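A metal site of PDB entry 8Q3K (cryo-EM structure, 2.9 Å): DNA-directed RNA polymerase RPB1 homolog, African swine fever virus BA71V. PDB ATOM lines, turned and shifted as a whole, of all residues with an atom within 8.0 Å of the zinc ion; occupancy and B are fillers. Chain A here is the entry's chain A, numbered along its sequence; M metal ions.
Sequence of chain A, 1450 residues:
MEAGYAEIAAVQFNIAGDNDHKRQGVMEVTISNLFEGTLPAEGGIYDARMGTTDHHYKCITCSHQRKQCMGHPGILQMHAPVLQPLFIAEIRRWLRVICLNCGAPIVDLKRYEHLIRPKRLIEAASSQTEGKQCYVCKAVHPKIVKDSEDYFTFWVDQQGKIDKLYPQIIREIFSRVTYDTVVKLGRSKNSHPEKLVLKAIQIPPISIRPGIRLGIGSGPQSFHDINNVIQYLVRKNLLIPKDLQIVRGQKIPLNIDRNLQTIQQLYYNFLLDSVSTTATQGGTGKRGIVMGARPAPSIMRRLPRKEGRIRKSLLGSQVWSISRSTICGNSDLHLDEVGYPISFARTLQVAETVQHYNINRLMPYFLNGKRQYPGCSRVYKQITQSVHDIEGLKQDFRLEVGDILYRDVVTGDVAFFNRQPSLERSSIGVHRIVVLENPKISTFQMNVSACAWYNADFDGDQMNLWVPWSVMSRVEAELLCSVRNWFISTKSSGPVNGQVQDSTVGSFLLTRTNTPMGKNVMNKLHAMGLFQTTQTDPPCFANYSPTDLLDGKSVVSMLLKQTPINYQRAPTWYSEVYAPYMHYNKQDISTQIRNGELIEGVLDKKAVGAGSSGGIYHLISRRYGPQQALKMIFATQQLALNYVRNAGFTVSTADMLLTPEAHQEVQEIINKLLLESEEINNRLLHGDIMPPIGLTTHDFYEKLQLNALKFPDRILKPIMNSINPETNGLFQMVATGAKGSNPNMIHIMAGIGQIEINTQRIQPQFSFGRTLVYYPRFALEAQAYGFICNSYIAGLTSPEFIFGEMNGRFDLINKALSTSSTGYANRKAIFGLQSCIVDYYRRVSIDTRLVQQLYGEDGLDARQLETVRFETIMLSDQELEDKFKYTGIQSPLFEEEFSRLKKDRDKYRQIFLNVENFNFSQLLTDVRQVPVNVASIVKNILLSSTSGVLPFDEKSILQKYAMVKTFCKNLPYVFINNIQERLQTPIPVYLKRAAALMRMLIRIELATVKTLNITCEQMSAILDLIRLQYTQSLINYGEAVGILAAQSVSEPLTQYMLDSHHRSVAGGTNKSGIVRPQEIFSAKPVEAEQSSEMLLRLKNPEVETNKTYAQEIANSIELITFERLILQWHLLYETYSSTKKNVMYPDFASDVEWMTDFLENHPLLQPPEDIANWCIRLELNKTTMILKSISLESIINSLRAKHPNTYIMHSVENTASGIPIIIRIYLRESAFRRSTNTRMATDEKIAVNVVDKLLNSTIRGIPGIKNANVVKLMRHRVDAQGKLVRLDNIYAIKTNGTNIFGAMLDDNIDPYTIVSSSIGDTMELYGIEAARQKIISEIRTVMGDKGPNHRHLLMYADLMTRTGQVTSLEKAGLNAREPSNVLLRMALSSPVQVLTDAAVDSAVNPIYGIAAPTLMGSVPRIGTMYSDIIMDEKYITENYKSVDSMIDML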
ATOM      1  N   ILE A  98      -5.771   8.719  20.796  1.00  0.00           N
ATOM      2  CA  ILE A  98      -5.441   8.297  22.158  1.00  0.00           C
ATOM      3  C   ILE A  98      -6.707   8.259  23.006  1.00  0.00           C
ATOM      4  O   ILE A  98      -7.564   9.139  22.889  1.00  0.00           O
ATOM      5  CB  ILE A  98      -4.393   9.236  22.785  1.00  0.00           C
ATOM      6  CG1 ILE A  98      -3.011   9.023  22.146  1.00  0.00           C
ATOM      7  CG2 ILE A  98      -4.306   9.015  24.288  1.00  0.00           C
ATOM      8  CD1 ILE A  98      -2.486   7.589  22.205  1.00  0.00           C
ATOM      9  N   CYS A  99      -6.806   7.251  23.869  1.00  0.00           N
ATOM     10  CA  CYS A  99      -7.908   7.169  24.820  1.00  0.00           C
ATOM     11  C   CYS A  99      -7.802   8.302  25.830  1.00  0.00           C
ATOM     12  O   CYS A  99      -6.717   8.570  26.365  1.00  0.00           O
ATOM     13  CB  CYS A  99      -7.897   5.815  25.537  1.00  0.00           C
ATOM     14  SG  CYS A  99      -8.985   5.682  26.988  1.00  0.00           S
ATOM     15  N   LEU A 100      -8.916   8.979  26.089  1.00  0.00           N
ATOM     16  CA  LEU A 100      -8.920  10.074  27.048  1.00  0.00           C
ATOM     17  C   LEU A 100      -8.856   9.566  28.486  1.00  0.00           C
ATOM     18  O   LEU A 100      -8.164  10.148  29.324  1.00  0.00           O
ATOM     19  CB  LEU A 100     -10.150  10.953  26.847  1.00  0.00           C
ATOM     20  CG  LEU A 100     -10.069  11.929  25.676  1.00  0.00           C
ATOM     21  CD1 LEU A 100     -10.006  11.205  24.343  1.00  0.00           C
ATOM     22  CD2 LEU A 100     -11.242  12.892  25.697  1.00  0.00           C
ATOM     23  N   ASN A 101      -9.571   8.481  28.780  1.00  0.00           N
ATOM     24  CA  ASN A 101      -9.598   7.971  30.159  1.00  0.00           C
ATOM     25  C   ASN A 101      -8.243   7.400  30.564  1.00  0.00           C
ATOM     26  O   ASN A 101      -7.788   7.626  31.686  1.00  0.00           O
ATOM     27  CB  ASN A 101     -10.691   6.917  30.295  1.00  0.00           C
ATOM     28  CG  ASN A 101     -10.869   6.445  31.722  1.00  0.00           C
ATOM     29  OD1 ASN A 101     -10.361   7.065  32.661  1.00  0.00           O
ATOM     30  ND2 ASN A 101     -11.612   5.358  31.891  1.00  0.00           N
ATOM     31  N   CYS A 102      -7.594   6.651  29.673  1.00  0.00           N
ATOM     32  CA  CYS A 102      -6.287   6.065  29.935  1.00  0.00           C
ATOM     33  C   CYS A 102      -5.376   6.301  28.743  1.00  0.00           C
ATOM     34  O   CYS A 102      -5.814   6.689  27.653  1.00  0.00           O
ATOM     35  CB  CYS A 102      -6.390   4.565  30.221  1.00  0.00           C
ATOM     36  SG  CYS A 102      -6.419   3.531  28.729  1.00  0.00           S
ATOM     37  N   GLY A 103      -4.084   6.050  28.950  1.00  0.00           N
ATOM     38  CA  GLY A 103      -3.097   6.300  27.915  1.00  0.00           C
ATOM     39  C   GLY A 103      -3.072   5.281  26.796  1.00  0.00           C
ATOM     40  O   GLY A 103      -2.378   5.511  25.798  1.00  0.00           O
ATOM     41  N   ALA A 104      -3.782   4.172  26.941  1.00  0.00           N
ATOM     42  CA  ALA A 104      -3.758   3.150  25.904  1.00  0.00           C
ATOM     43  C   ALA A 104      -4.351   3.698  24.608  1.00  0.00           C
ATOM     44  O   ALA A 104      -5.323   4.463  24.643  1.00  0.00           O
ATOM     45  CB  ALA A 104      -4.532   1.907  26.350  1.00  0.00           C
ATOM     46  N   PRO A 105      -3.788   3.350  23.454  1.00  0.00           N
ATOM     47  CA  PRO A 105      -4.360   3.825  22.192  1.00  0.00           C
ATOM     48  C   PRO A 105      -5.713   3.189  21.911  1.00  0.00           C
ATOM     49  O   PRO A 105      -5.998   2.073  22.329  1.00  0.00           O
ATOM     50  CB  PRO A 105      -3.325   3.395  21.147  1.00  0.00           C
ATOM     51  CG  PRO A 105      -2.654   2.216  21.752  1.00  0.00           C
ATOM     52  CD  PRO A 105      -2.616   2.478  23.236  1.00  0.00           C
ATOM     53  N   ILE A 106      -6.550   3.938  21.186  1.00  0.00           N
ATOM     54  CA  ILE A 106      -7.853   3.433  20.759  1.00  0.00           C
ATOM     55  C   ILE A 106      -7.818   2.832  19.372  1.00  0.00           C
ATOM     56  O   ILE A 106      -8.864   2.463  18.832  1.00  0.00           O
ATOM     57  CB  ILE A 106      -8.923   4.546  20.826  1.00  0.00           C
ATOM     58  CG1 ILE A 106      -8.723   5.553  19.686  1.00  0.00           C
ATOM     59  CG2 ILE A 106      -8.896   5.231  22.175  1.00  0.00           C
ATOM     60  CD1 ILE A 106      -9.761   6.640  19.657  1.00  0.00           C
ATOM     61  N   GLN A 133     -14.469   1.995  21.367  1.00  0.00           N
ATOM     62  CA  GLN A 133     -14.458   1.807  22.810  1.00  0.00           C
ATOM     63  C   GLN A 133     -13.099   1.263  23.233  1.00  0.00           C
ATOM     64  O   GLN A 133     -12.601   0.312  22.628  1.00  0.00           O
ATOM     65  CB  GLN A 133     -15.576   0.858  23.243  1.00  0.00           C
ATOM     66  CG  GLN A 133     -15.488   0.398  24.691  1.00  0.00           C
ATOM     67  CD  GLN A 133     -16.785  -0.208  25.188  1.00  0.00           C
ATOM     68  OE1 GLN A 133     -17.812  -0.134  24.514  1.00  0.00           O
ATOM     69  NE2 GLN A 133     -16.748  -0.806  26.364  1.00  0.00           N
ATOM     70  N   CYS A 134     -12.511   1.871  24.263  1.00  0.00           N
ATOM     71  CA  CYS A 134     -11.200   1.469  24.724  1.00  0.00           C
ATOM     72  C   CYS A 134     -11.246   0.058  25.303  1.00  0.00           C
ATOM     73  O   CYS A 134     -12.224  -0.343  25.942  1.00  0.00           O
ATOM     74  CB  CYS A 134     -10.683   2.460  25.770  1.00  0.00           C
ATOM     75  SG  CYS A 134      -9.276   1.898  26.754  1.00  0.00           S
ATOM     76  N   TYR A 135     -10.182  -0.717  25.050  1.00  0.00           N
ATOM     77  CA  TYR A 135     -10.143  -2.086  25.544  1.00  0.00           C
ATOM     78  C   TYR A 135     -10.086  -2.129  27.060  1.00  0.00           C
ATOM     79  O   TYR A 135     -10.792  -2.920  27.698  1.00  0.00           O
ATOM     80  CB  TYR A 135      -8.959  -2.832  24.935  1.00  0.00           C
ATOM     81  CG  TYR A 135      -8.988  -4.337  25.112  1.00  0.00           C
ATOM     82  CD1 TYR A 135     -10.124  -4.990  25.584  1.00  0.00           C
ATOM     83  CD2 TYR A 135      -7.881  -5.118  24.804  1.00  0.00           C
ATOM     84  CE1 TYR A 135     -10.152  -6.367  25.749  1.00  0.00           C
ATOM     85  CE2 TYR A 135      -7.899  -6.489  24.950  1.00  0.00           C
ATOM     86  CZ  TYR A 135      -9.029  -7.106  25.427  1.00  0.00           C
ATOM     87  OH  TYR A 135      -9.055  -8.476  25.581  1.00  0.00           O
ATOM     88  N   VAL A 136      -9.245  -1.296  27.668  1.00  0.00           N
ATOM     89  CA  VAL A 136      -9.107  -1.298  29.123  1.00  0.00           C
ATOM     90  C   VAL A 136     -10.047  -0.307  29.802  1.00  0.00           C
ATOM     91  O   VAL A 136     -10.266  -0.416  31.009  1.00  0.00           O
ATOM     92  CB  VAL A 136      -7.653  -1.009  29.543  1.00  0.00           C
ATOM     93  CG1 VAL A 136      -6.681  -1.862  28.728  1.00  0.00           C
ATOM     94  CG2 VAL A 136      -7.319   0.466  29.383  1.00  0.00           C
ATOM     95  N   CYS A 137     -10.606   0.640  29.055  1.00  0.00           N
ATOM     96  CA  CYS A 137     -11.604   1.568  29.566  1.00  0.00           C
ATOM     97  C   CYS A 137     -12.921   1.320  28.834  1.00  0.00           C
ATOM     98  O   CYS A 137     -12.954   1.289  27.604  1.00  0.00           O
ATOM     99  CB  CYS A 137     -11.183   3.019  29.365  1.00  0.00           C
ATOM    100  SG  CYS A 137      -9.699   3.512  30.245  1.00  0.00           S
ATOM    101  N   LYS A 138     -13.992   1.158  29.605  1.00  0.00           N
ATOM    102  CA  LYS A 138     -15.309   1.048  28.985  1.00  0.00           C
ATOM    103  C   LYS A 138     -15.751   2.343  28.323  1.00  0.00           C
ATOM    104  O   LYS A 138     -16.736   2.333  27.579  1.00  0.00           O
ATOM    105  CB  LYS A 138     -16.350   0.615  30.022  1.00  0.00           C
ATOM    106  CG  LYS A 138     -16.165  -0.814  30.504  1.00  0.00           C
ATOM    107  CD  LYS A 138     -17.336  -1.273  31.359  1.00  0.00           C
ATOM    108  CE  LYS A 138     -17.222  -2.746  31.717  1.00  0.00           C
ATOM    109  NZ  LYS A 138     -18.370  -3.211  32.539  1.00  0.00           N
ATOM    110  N   ALA A 139     -15.044   3.446  28.578  1.00  0.00           N
ATOM    111  CA  ALA A 139     -15.389   4.708  27.956  1.00  0.00           C
ATOM    112  C   ALA A 139     -15.299   4.619  26.442  1.00  0.00           C
ATOM    113  O   ALA A 139     -14.395   3.986  25.896  1.00  0.00           O
ATOM    114  CB  ALA A 139     -14.465   5.809  28.476  1.00  0.00           C
ATOM    115  N   ARG A 176      -0.655  10.370  30.678  1.00  0.00           N
ATOM    116  CA  ARG A 176      -0.800   8.932  30.868  1.00  0.00           C
ATOM    117  C   ARG A 176      -0.350   8.121  29.660  1.00  0.00           C
ATOM    118  O   ARG A 176      -0.218   6.896  29.771  1.00  0.00           O
ATOM    119  CB  ARG A 176      -2.255   8.576  31.199  1.00  0.00           C
ATOM    120  CG  ARG A 176      -3.030   9.689  31.898  1.00  0.00           C
ATOM    121  CD  ARG A 176      -4.370   9.190  32.396  1.00  0.00           C
ATOM    122  NE  ARG A 176      -5.261  10.304  32.747  1.00  0.00           N
ATOM    123  CZ  ARG A 176      -6.097  10.880  31.897  1.00  0.00           C
ATOM    124  NH1 ARG A 176      -6.204  10.485  30.638  1.00  0.00           N
ATOM    125  NH2 ARG A 176      -6.852  11.887  32.324  1.00  0.00           N
HETATM  126 ZN    ZN M   1      -8.669   3.675  28.153  1.00  0.00          ZN
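SG of Cys 102 lies close to N of Ala 104 (3.2 Å).
The side-chain sulfur (SG) of Cys 137 sits close to the side-chain amide nitrogen (ND2) of Asn 101, 3.1 Å away.
The backbone NH of Val 136 lies close to the side-chain sulfur of Cys 134 (3.3 Å).
N of Cys 134 sits at hydrogen-bond distance from O of Ala 139, 3.3 Å away.
The backbone NH of Asn 101 sits close to the side-chain sulfur of Cys 99.
The backbone carbonyl oxygen (O) of Ala 104 sits close to the backbone NH (N) of Cys 99, at 3.3 Å.
Merely in contact with the zinc ion: Val 136.
The side-chain sulfur (SG) of Cys 102 binds the zinc ion (2.3 Å).
The zinc ion is bound by the side-chain sulfur (SG) of Cys 137 (2.3 Å).
SG of Cys 134 is bound to the zinc ion (2.3 Å).
SG of Cys 99 binds the zinc ion (2.3 Å).
The zinc ion has four donor atoms within binding distance.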
